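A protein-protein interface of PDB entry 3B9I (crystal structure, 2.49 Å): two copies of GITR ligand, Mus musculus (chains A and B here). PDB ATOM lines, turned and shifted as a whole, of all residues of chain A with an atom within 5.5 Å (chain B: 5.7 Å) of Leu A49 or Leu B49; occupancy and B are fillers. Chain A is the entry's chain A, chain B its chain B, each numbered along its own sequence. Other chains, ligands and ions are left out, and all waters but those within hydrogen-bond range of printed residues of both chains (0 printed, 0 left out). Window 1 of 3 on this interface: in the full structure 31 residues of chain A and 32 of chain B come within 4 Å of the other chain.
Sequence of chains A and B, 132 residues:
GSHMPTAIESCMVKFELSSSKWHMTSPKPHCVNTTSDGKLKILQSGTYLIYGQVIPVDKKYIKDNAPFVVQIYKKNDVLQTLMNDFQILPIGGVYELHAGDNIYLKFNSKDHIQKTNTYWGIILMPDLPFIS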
ATOM      1  N   MET A  12     -14.533 -19.723 -18.839  1.00  0.00           N
ATOM      2  CA  MET A  12     -13.239 -20.132 -19.328  1.00  0.00           C
ATOM      3  C   MET A  12     -13.251 -20.365 -20.850  1.00  0.00           C
ATOM      4  O   MET A  12     -14.229 -20.883 -21.413  1.00  0.00           O
ATOM      5  CB  MET A  12     -12.781 -21.381 -18.561  1.00  0.00           C
ATOM      6  CG  MET A  12     -11.668 -22.116 -19.244  1.00  0.00           C
ATOM      7  SD  MET A  12     -10.898 -23.451 -18.305  1.00  0.00           S
ATOM      8  CE  MET A  12      -9.380 -23.617 -19.247  1.00  0.00           C
ATOM      9  N   THR A  47     -10.178 -11.573 -10.893  1.00  0.00           N
ATOM     10  CA  THR A  47      -8.907 -12.238 -10.909  1.00  0.00           C
ATOM     11  C   THR A  47      -8.948 -13.297 -11.993  1.00  0.00           C
ATOM     12  O   THR A  47      -9.817 -14.185 -11.997  1.00  0.00           O
ATOM     13  CB  THR A  47      -8.635 -12.877  -9.566  1.00  0.00           C
ATOM     14  OG1 THR A  47      -8.753 -11.861  -8.569  1.00  0.00           O
ATOM     15  CG2 THR A  47      -7.243 -13.432  -9.519  1.00  0.00           C
ATOM     16  N   TYR A  48      -8.016 -13.191 -12.922  1.00  0.00           N
ATOM     17  CA  TYR A  48      -7.996 -14.102 -14.046  1.00  0.00           C
ATOM     18  C   TYR A  48      -6.704 -14.887 -14.118  1.00  0.00           C
ATOM     19  O   TYR A  48      -5.632 -14.390 -13.771  1.00  0.00           O
ATOM     20  CB  TYR A  48      -8.180 -13.329 -15.340  1.00  0.00           C
ATOM     21  CG  TYR A  48      -9.587 -12.868 -15.612  1.00  0.00           C
ATOM     22  CD1 TYR A  48     -10.411 -13.591 -16.453  1.00  0.00           C
ATOM     23  CD2 TYR A  48     -10.082 -11.697 -15.057  1.00  0.00           C
ATOM     24  CE1 TYR A  48     -11.705 -13.166 -16.728  1.00  0.00           C
ATOM     25  CE2 TYR A  48     -11.369 -11.265 -15.318  1.00  0.00           C
ATOM     26  CZ  TYR A  48     -12.172 -12.003 -16.152  1.00  0.00           C
ATOM     27  OH  TYR A  48     -13.449 -11.604 -16.438  1.00  0.00           O
ATOM     28  N   LEU A  49      -6.812 -16.128 -14.563  1.00  0.00           N
ATOM     29  CA  LEU A  49      -5.632 -16.892 -14.905  1.00  0.00           C
ATOM     30  C   LEU A  49      -5.514 -16.934 -16.431  1.00  0.00           C
ATOM     31  O   LEU A  49      -6.338 -17.551 -17.102  1.00  0.00           O
ATOM     32  CB  LEU A  49      -5.715 -18.304 -14.307  1.00  0.00           C
ATOM     33  CG  LEU A  49      -4.640 -19.362 -14.606  1.00  0.00           C
ATOM     34  CD1 LEU A  49      -3.228 -18.883 -14.213  1.00  0.00           C
ATOM     35  CD2 LEU A  49      -4.993 -20.651 -13.891  1.00  0.00           C
ATOM     36  N   ILE A  50      -4.509 -16.241 -16.963  1.00  0.00           N
ATOM     37  CA  ILE A  50      -4.120 -16.346 -18.370  1.00  0.00           C
ATOM     38  C   ILE A  50      -3.152 -17.510 -18.482  1.00  0.00           C
ATOM     39  O   ILE A  50      -2.165 -17.582 -17.733  1.00  0.00           O
ATOM     40  CB  ILE A  50      -3.371 -15.064 -18.853  1.00  0.00           C
ATOM     41  CG1 ILE A  50      -4.247 -13.822 -18.689  1.00  0.00           C
ATOM     42  CG2 ILE A  50      -2.831 -15.213 -20.304  1.00  0.00           C
ATOM     43  CD1 ILE A  50      -3.473 -12.510 -18.817  1.00  0.00           C
ATOM     44  N   TYR A  51      -3.424 -18.408 -19.418  1.00  0.00           N
ATOM     45  CA  TYR A  51      -2.602 -19.592 -19.625  1.00  0.00           C
ATOM     46  C   TYR A  51      -2.384 -19.819 -21.097  1.00  0.00           C
ATOM     47  O   TYR A  51      -2.986 -19.152 -21.922  1.00  0.00           O
ATOM     48  CB  TYR A  51      -3.289 -20.834 -19.054  1.00  0.00           C
ATOM     49  CG  TYR A  51      -4.559 -21.199 -19.791  1.00  0.00           C
ATOM     50  CD1 TYR A  51      -4.575 -22.227 -20.743  1.00  0.00           C
ATOM     51  CD2 TYR A  51      -5.751 -20.528 -19.531  1.00  0.00           C
ATOM     52  CE1 TYR A  51      -5.751 -22.572 -21.422  1.00  0.00           C
ATOM     53  CE2 TYR A  51      -6.929 -20.869 -20.198  1.00  0.00           C
ATOM     54  CZ  TYR A  51      -6.924 -21.884 -21.143  1.00  0.00           C
ATOM     55  OH  TYR A  51      -8.100 -22.201 -21.792  1.00  0.00           O
ATOM     56  N   GLY A  92       1.661 -16.938 -19.101  1.00  0.00           N
ATOM     57  CA  GLY A  92       0.550 -16.429 -18.322  1.00  0.00           C
ATOM     58  C   GLY A  92       0.832 -16.405 -16.837  1.00  0.00           C
ATOM     59  O   GLY A  92       1.987 -16.452 -16.408  1.00  0.00           O
ATOM     60  N   GLY A  93      -0.244 -16.353 -16.052  1.00  0.00           N
ATOM     61  CA  GLY A  93      -0.154 -16.273 -14.616  1.00  0.00           C
ATOM     62  C   GLY A  93      -1.439 -15.656 -14.110  1.00  0.00           C
ATOM     63  O   GLY A  93      -2.403 -15.457 -14.872  1.00  0.00           O
ATOM     64  N   VAL A  94      -1.457 -15.351 -12.820  1.00  0.00           N
ATOM     65  CA  VAL A  94      -2.615 -14.721 -12.226  1.00  0.00           C
ATOM     66  C   VAL A  94      -2.461 -13.207 -12.372  1.00  0.00           C
ATOM     67  O   VAL A  94      -1.445 -12.647 -11.950  1.00  0.00           O
ATOM     68  CB  VAL A  94      -2.763 -15.130 -10.748  1.00  0.00           C
ATOM     69  CG1 VAL A  94      -3.826 -14.290 -10.061  1.00  0.00           C
ATOM     70  CG2 VAL A  94      -3.101 -16.605 -10.658  1.00  0.00           C
ATOM     71  N   TYR A  95      -3.449 -12.569 -13.011  1.00  0.00           N
ATOM     72  CA  TYR A  95      -3.491 -11.113 -13.212  1.00  0.00           C
ATOM     73  C   TYR A  95      -4.854 -10.514 -12.826  1.00  0.00           C
ATOM     74  O   TYR A  95      -5.919 -11.129 -13.033  1.00  0.00           O
ATOM     75  CB  TYR A  95      -3.145 -10.752 -14.665  1.00  0.00           C
ATOM     76  CG  TYR A  95      -1.752 -11.141 -15.009  1.00  0.00           C
ATOM     77  CD1 TYR A  95      -0.687 -10.302 -14.701  1.00  0.00           C
ATOM     78  CD2 TYR A  95      -1.478 -12.378 -15.588  1.00  0.00           C
ATOM     79  CE1 TYR A  95       0.625 -10.674 -14.980  1.00  0.00           C
ATOM     80  CE2 TYR A  95      -0.173 -12.766 -15.874  1.00  0.00           C
ATOM     81  CZ  TYR A  95       0.870 -11.907 -15.566  1.00  0.00           C
ATOM     82  OH  TYR A  95       2.159 -12.269 -15.852  1.00  0.00           O
ATOM     83  N   GLY A 121      -5.487 -18.927 -23.451  1.00  0.00           N
ATOM     84  CA  GLY A 121      -6.810 -18.489 -23.002  1.00  0.00           C
ATOM     85  C   GLY A 121      -6.837 -17.868 -21.611  1.00  0.00           C
ATOM     86  O   GLY A 121      -5.791 -17.536 -21.058  1.00  0.00           O
ATOM     87  N   ILE A 122      -8.039 -17.698 -21.055  1.00  0.00           N
ATOM     88  CA  ILE A 122      -8.199 -17.235 -19.685  1.00  0.00           C
ATOM     89  C   ILE A 122      -9.269 -18.029 -18.976  1.00  0.00           C
ATOM     90  O   ILE A 122     -10.166 -18.600 -19.595  1.00  0.00           O
ATOM     91  CB  ILE A 122      -8.668 -15.754 -19.558  1.00  0.00           C
ATOM     92  CG1 ILE A 122      -9.774 -15.461 -20.564  1.00  0.00           C
ATOM     93  CG2 ILE A 122      -7.548 -14.791 -19.719  1.00  0.00           C
ATOM     94  CD1 ILE A 122     -10.803 -14.478 -20.091  1.00  0.00           C
ATOM     95  N   ILE A 123      -9.162 -18.021 -17.656  1.00  0.00           N
ATOM     96  CA  ILE A 123     -10.202 -18.500 -16.775  1.00  0.00           C
ATOM     97  C   ILE A 123     -10.403 -17.483 -15.646  1.00  0.00           C
ATOM     98  O   ILE A 123      -9.438 -17.090 -14.983  1.00  0.00           O
ATOM     99  CB  ILE A 123      -9.914 -19.946 -16.246  1.00  0.00           C
ATOM    100  CG1 ILE A 123     -10.789 -20.266 -15.033  1.00  0.00           C
ATOM    101  CG2 ILE A 123      -8.447 -20.143 -15.920  1.00  0.00           C
ATOM    102  CD1 ILE A 123     -11.388 -21.675 -15.084  1.00  0.00           C
ATOM    103  N   LEU A 124     -11.649 -17.010 -15.504  1.00  0.00           N
ATOM    104  CA  LEU A 124     -12.072 -16.197 -14.360  1.00  0.00           C
ATOM    105  C   LEU A 124     -11.866 -17.039 -13.131  1.00  0.00           C
ATOM    106  O   LEU A 124     -12.452 -18.096 -13.012  1.00  0.00           O
ATOM    107  CB  LEU A 124     -13.550 -15.842 -14.459  1.00  0.00           C
ATOM    108  CG  LEU A 124     -14.175 -14.965 -13.362  1.00  0.00           C
ATOM    109  CD1 LEU A 124     -13.425 -13.640 -13.117  1.00  0.00           C
ATOM    110  CD2 LEU A 124     -15.655 -14.662 -13.670  1.00  0.00           C
ATOM    111  N   MET A 125     -11.005 -16.611 -12.227  1.00  0.00           N
ATOM    112  CA  MET A 125     -10.791 -17.414 -11.035  1.00  0.00           C
ATOM    113  C   MET A 125     -11.828 -17.149  -9.928  1.00  0.00           C
ATOM    114  O   MET A 125     -12.245 -16.014  -9.712  1.00  0.00           O
ATOM    115  CB  MET A 125      -9.395 -17.192 -10.489  1.00  0.00           C
ATOM    116  CG  MET A 125      -8.322 -17.807 -11.317  1.00  0.00           C
ATOM    117  SD  MET A 125      -6.769 -17.099 -10.761  1.00  0.00           S
ATOM    118  CE  MET A 125      -6.901 -17.195  -8.954  1.00  0.00           C
ATOM    119  N   MET B  12      -9.926 -25.125  -6.991  1.00  0.00           N
ATOM    120  CA  MET B  12      -8.670 -24.472  -7.312  1.00  0.00           C
ATOM    121  C   MET B  12      -7.833 -24.275  -6.067  1.00  0.00           C
ATOM    122  O   MET B  12      -8.356 -23.934  -5.000  1.00  0.00           O
ATOM    123  CB  MET B  12      -8.921 -23.105  -7.951  1.00  0.00           C
ATOM    124  CG  MET B  12      -7.645 -22.469  -8.492  1.00  0.00           C
ATOM    125  SD  MET B  12      -7.851 -20.814  -9.200  1.00  0.00           S
ATOM    126  CE  MET B  12      -6.266 -20.565  -9.999  1.00  0.00           C
ATOM    127  N   THR B  47      -9.338 -33.152 -16.466  1.00  0.00           N
ATOM    128  CA  THR B  47      -8.456 -32.216 -17.146  1.00  0.00           C
ATOM    129  C   THR B  47      -8.058 -31.121 -16.171  1.00  0.00           C
ATOM    130  O   THR B  47      -8.903 -30.449 -15.570  1.00  0.00           O
ATOM    131  CB  THR B  47      -9.150 -31.529 -18.345  1.00  0.00           C
ATOM    132  OG1 THR B  47      -9.933 -32.486 -19.063  1.00  0.00           O
ATOM    133  CG2 THR B  47      -8.123 -30.897 -19.288  1.00  0.00           C
ATOM    134  N   TYR B  48      -6.763 -30.918 -16.038  1.00  0.00           N
ATOM    135  CA  TYR B  48      -6.285 -29.900 -15.137  1.00  0.00           C
ATOM    136  C   TYR B  48      -5.432 -28.876 -15.851  1.00  0.00           C
ATOM    137  O   TYR B  48      -4.769 -29.171 -16.854  1.00  0.00           O
ATOM    138  CB  TYR B  48      -5.483 -30.533 -14.000  1.00  0.00           C
ATOM    139  CG  TYR B  48      -6.340 -31.182 -12.941  1.00  0.00           C
ATOM    140  CD1 TYR B  48      -6.650 -30.508 -11.764  1.00  0.00           C
ATOM    141  CD2 TYR B  48      -6.839 -32.468 -13.113  1.00  0.00           C
ATOM    142  CE1 TYR B  48      -7.447 -31.100 -10.781  1.00  0.00           C
ATOM    143  CE2 TYR B  48      -7.644 -33.067 -12.140  1.00  0.00           C
ATOM    144  CZ  TYR B  48      -7.939 -32.380 -10.976  1.00  0.00           C
ATOM    145  OH  TYR B  48      -8.717 -32.968  -9.999  1.00  0.00           O
ATOM    146  N   LEU B  49      -5.466 -27.660 -15.317  1.00  0.00           N
ATOM    147  CA  LEU B  49      -4.527 -26.628 -15.694  1.00  0.00           C
ATOM    148  C   LEU B  49      -3.569 -26.462 -14.546  1.00  0.00           C
ATOM    149  O   LEU B  49      -3.951 -26.013 -13.464  1.00  0.00           O
ATOM    150  CB  LEU B  49      -5.265 -25.320 -15.993  1.00  0.00           C
ATOM    151  CG  LEU B  49      -4.475 -24.053 -16.312  1.00  0.00           C
ATOM    152  CD1 LEU B  49      -3.382 -24.230 -17.408  1.00  0.00           C
ATOM    153  CD2 LEU B  49      -5.466 -22.970 -16.690  1.00  0.00           C
ATOM    154  N   ILE B  50      -2.332 -26.896 -14.767  1.00  0.00           N
ATOM    155  CA  ILE B  50      -1.262 -26.682 -13.808  1.00  0.00           C
ATOM    156  C   ILE B  50      -0.694 -25.345 -14.200  1.00  0.00           C
ATOM    157  O   ILE B  50      -0.446 -25.125 -15.375  1.00  0.00           O
ATOM    158  CB  ILE B  50      -0.145 -27.738 -13.957  1.00  0.00           C
ATOM    159  CG1 ILE B  50      -0.695 -29.147 -13.736  1.00  0.00           C
ATOM    160  CG2 ILE B  50       1.047 -27.440 -13.009  1.00  0.00           C
ATOM    161  CD1 ILE B  50       0.327 -30.222 -14.008  1.00  0.00           C
ATOM    162  N   TYR B  51      -0.496 -24.454 -13.236  1.00  0.00           N
ATOM    163  CA  TYR B  51       0.024 -23.125 -13.542  1.00  0.00           C
ATOM    164  C   TYR B  51       0.991 -22.713 -12.463  1.00  0.00           C
ATOM    165  O   TYR B  51       1.157 -23.406 -11.466  1.00  0.00           O
ATOM    166  CB  TYR B  51      -1.116 -22.098 -13.594  1.00  0.00           C
ATOM    167  CG  TYR B  51      -1.753 -21.867 -12.238  1.00  0.00           C
ATOM    168  CD1 TYR B  51      -1.455 -20.716 -11.498  1.00  0.00           C
ATOM    169  CD2 TYR B  51      -2.639 -22.803 -11.687  1.00  0.00           C
ATOM    170  CE1 TYR B  51      -2.019 -20.497 -10.256  1.00  0.00           C
ATOM    171  CE2 TYR B  51      -3.213 -22.596 -10.429  1.00  0.00           C
ATOM    172  CZ  TYR B  51      -2.901 -21.442  -9.720  1.00  0.00           C
ATOM    173  OH  TYR B  51      -3.455 -21.215  -8.481  1.00  0.00           O
ATOM    174  N   GLY B  92       3.609 -24.881 -16.480  1.00  0.00           N
ATOM    175  CA  GLY B  92       2.407 -25.690 -16.588  1.00  0.00           C
ATOM    176  C   GLY B  92       1.729 -25.762 -17.941  1.00  0.00           C
ATOM    177  O   GLY B  92       2.384 -25.760 -18.988  1.00  0.00           O
ATOM    178  N   GLY B  93       0.398 -25.828 -17.893  1.00  0.00           N
ATOM    179  CA  GLY B  93      -0.433 -26.048 -19.055  1.00  0.00           C
ATOM    180  C   GLY B  93      -1.544 -27.024 -18.708  1.00  0.00           C
ATOM    181  O   GLY B  93      -1.697 -27.430 -17.550  1.00  0.00           O
ATOM    182  N   VAL B  94      -2.318 -27.395 -19.723  1.00  0.00           N
ATOM    183  CA  VAL B  94      -3.423 -28.334 -19.593  1.00  0.00           C
ATOM    184  C   VAL B  94      -2.935 -29.788 -19.685  1.00  0.00           C
ATOM    185  O   VAL B  94      -2.245 -30.167 -20.650  1.00  0.00           O
ATOM    186  CB  VAL B  94      -4.487 -28.072 -20.690  1.00  0.00           C
ATOM    187  CG1 VAL B  94      -5.580 -29.090 -20.618  1.00  0.00           C
ATOM    188  CG2 VAL B  94      -5.068 -26.696 -20.541  1.00  0.00           C
ATOM    189  N   TYR B  95      -3.289 -30.582 -18.674  1.00  0.00           N
ATOM    190  CA  TYR B  95      -2.929 -32.007 -18.593  1.00  0.00           C
ATOM    191  C   TYR B  95      -4.077 -32.883 -18.062  1.00  0.00           C
ATOM    192  O   TYR B  95      -4.739 -32.536 -17.070  1.00  0.00           O
ATOM    193  CB  TYR B  95      -1.718 -32.216 -17.675  1.00  0.00           C
ATOM    194  CG  TYR B  95      -0.464 -31.536 -18.141  1.00  0.00           C
ATOM    195  CD1 TYR B  95       0.384 -32.146 -19.074  1.00  0.00           C
ATOM    196  CD2 TYR B  95      -0.128 -30.274 -17.664  1.00  0.00           C
ATOM    197  CE1 TYR B  95       1.521 -31.521 -19.508  1.00  0.00           C
ATOM    198  CE2 TYR B  95       1.013 -29.636 -18.088  1.00  0.00           C
ATOM    199  CZ  TYR B  95       1.835 -30.263 -19.005  1.00  0.00           C
ATOM    200  OH  TYR B  95       2.967 -29.601 -19.419  1.00  0.00           O
ATOM    201  N   GLY B 121      -0.022 -23.932  -8.571  1.00  0.00           N
ATOM    202  CA  GLY B 121      -1.123 -24.723  -8.086  1.00  0.00           C
ATOM    203  C   GLY B 121      -1.860 -25.286  -9.274  1.00  0.00           C
ATOM    204  O   GLY B 121      -1.301 -25.358 -10.368  1.00  0.00           O
ATOM    205  N   ILE B 122      -3.115 -25.677  -9.072  1.00  0.00           N
ATOM    206  CA  ILE B 122      -3.887 -26.280 -10.143  1.00  0.00           C
ATOM    207  C   ILE B 122      -5.323 -25.818 -10.104  1.00  0.00           C
ATOM    208  O   ILE B 122      -5.799 -25.320  -9.092  1.00  0.00           O
ATOM    209  CB  ILE B 122      -3.850 -27.852 -10.139  1.00  0.00           C
ATOM    210  CG1 ILE B 122      -4.158 -28.432  -8.776  1.00  0.00           C
ATOM    211  CG2 ILE B 122      -2.524 -28.401 -10.577  1.00  0.00           C
ATOM    212  CD1 ILE B 122      -5.592 -28.722  -8.560  1.00  0.00           C
ATOM    213  N   ILE B 123      -5.996 -25.967 -11.234  1.00  0.00           N
ATOM    214  CA  ILE B 123      -7.440 -25.829 -11.289  1.00  0.00           C
ATOM    215  C   ILE B 123      -8.027 -26.986 -12.110  1.00  0.00           C
ATOM    216  O   ILE B 123      -7.546 -27.308 -13.216  1.00  0.00           O
ATOM    217  CB  ILE B 123      -7.897 -24.410 -11.798  1.00  0.00           C
ATOM    218  CG1 ILE B 123      -9.379 -24.401 -12.210  1.00  0.00           C
ATOM    219  CG2 ILE B 123      -7.040 -23.930 -12.929  1.00  0.00           C
ATOM    220  CD1 ILE B 123     -10.188 -23.138 -11.705  1.00  0.00           C
ATOM    221  N   LEU B 124      -9.030 -27.644 -11.526  1.00  0.00           N
ATOM    222  CA  LEU B 124      -9.796 -28.638 -12.239  1.00  0.00           C
ATOM    223  C   LEU B 124     -10.608 -27.911 -13.300  1.00  0.00           C
ATOM    224  O   LEU B 124     -11.340 -26.977 -12.988  1.00  0.00           O
ATOM    225  CB  LEU B 124     -10.726 -29.386 -11.286  1.00  0.00           C
ATOM    226  CG  LEU B 124     -11.780 -30.269 -11.978  1.00  0.00           C
ATOM    227  CD1 LEU B 124     -11.134 -31.421 -12.777  1.00  0.00           C
ATOM    228  CD2 LEU B 124     -12.802 -30.775 -10.961  1.00  0.00           C
ATOM    229  N   MET B 125     -10.460 -28.332 -14.550  1.00  0.00           N
ATOM    230  CA  MET B 125     -11.074 -27.627 -15.661  1.00  0.00           C
ATOM    231  C   MET B 125     -12.460 -28.134 -16.032  1.00  0.00           C
ATOM    232  O   MET B 125     -12.687 -29.335 -16.102  1.00  0.00           O
ATOM    233  CB  MET B 125     -10.171 -27.696 -16.891  1.00  0.00           C
ATOM    234  CG  MET B 125      -9.210 -26.531 -16.987  1.00  0.00           C
ATOM    235  SD  MET B 125      -8.026 -26.761 -18.311  1.00  0.00           S
ATOM    236  CE  MET B 125      -9.046 -26.863 -19.804  1.00  0.00           C
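The backbone carbonyl oxygen (O) of Tyr A51 is in hydrogen-bond range of the backbone NH (N) of Gly A121, 2.9 Å away. O of Thr B47 sits at hydrogen-bond distance from N of Met B125, at 2.8 Å. N of Leu B49 lies within hydrogen-bond range of O of Ile B123 (3.0 Å). N of Leu A49 sits at hydrogen-bond distance from O of Ile A123. N of Met A125 lies within hydrogen-bond range of O of Thr A47, at 2.7 Å. O of Gly B121 is in hydrogen-bond range of N of Tyr B51, at 3.1 Å.
Met B125 touches Met A12. CD2 of Leu A49 touches CD2 of Leu B49, 3.7 Å away. Tyr B51 touches Leu A49 (CD1 to CD1, 3.7 Å). CG2 of Ile B123 touches CD2 of Leu A49 (3.98 Å). CG of Tyr A51 touches CD2 of Leu B49, at 3.7 Å. Ile A123 touches Ile B123. CE of Met B12 touches SD of Met A125, at 3.6 Å.
Printed residues of chain B within 4 Å of Leu A49: Leu B49 (3.7 Å), Tyr B51 (3.7 Å) and Ile B123 (3.98 Å). Printed residues of chain A within 4 Å of Leu B49: Leu A49 and Tyr A51. Of the printed residues of chain B, Met A12 touches Met B125. Printed residues of chain A within 4 Å of Met B12: Met A125. Of the printed residues of chain A, Met B125 touches Met A12 (3.3 Å). Of the printed residues of chain B, Ile A123 touches Ile B123 (3.9 Å). Of the printed residues of chain B, Tyr A51 touches Leu B49. Val A94 touches none of the printed residues of chain B. The nearest printed residue of chain B that does not touch Met A125 is Tyr B51 (5.3 Å).
Printed residues of chain B that touch a printed residue of chain A: Met B12, Leu B49, Tyr B51, Ile B123 and Met B125. Along chain B the printed residues that touch a printed residue of chain A span positions 12 to 125. Of the 15 printed residues of chain A, 5 touch a printed residue of chain B. Among the printed residues, 7 pairs touch across the chains.
Met A12 touches Met B125, and with the chains exchanged Met A125 touches Met B12. Leu A49 touches its own counterpart, Leu B49. Leu A49 touches Ile B123, but with the chains exchanged Ile A123 does not touch Leu B49 (4.2 Å). Ile B123 touches its own counterpart, Ile A123. Of the 7 pairs that touch across the chains among the printed residues, 6 have their exchanged pair printed and touching as well.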
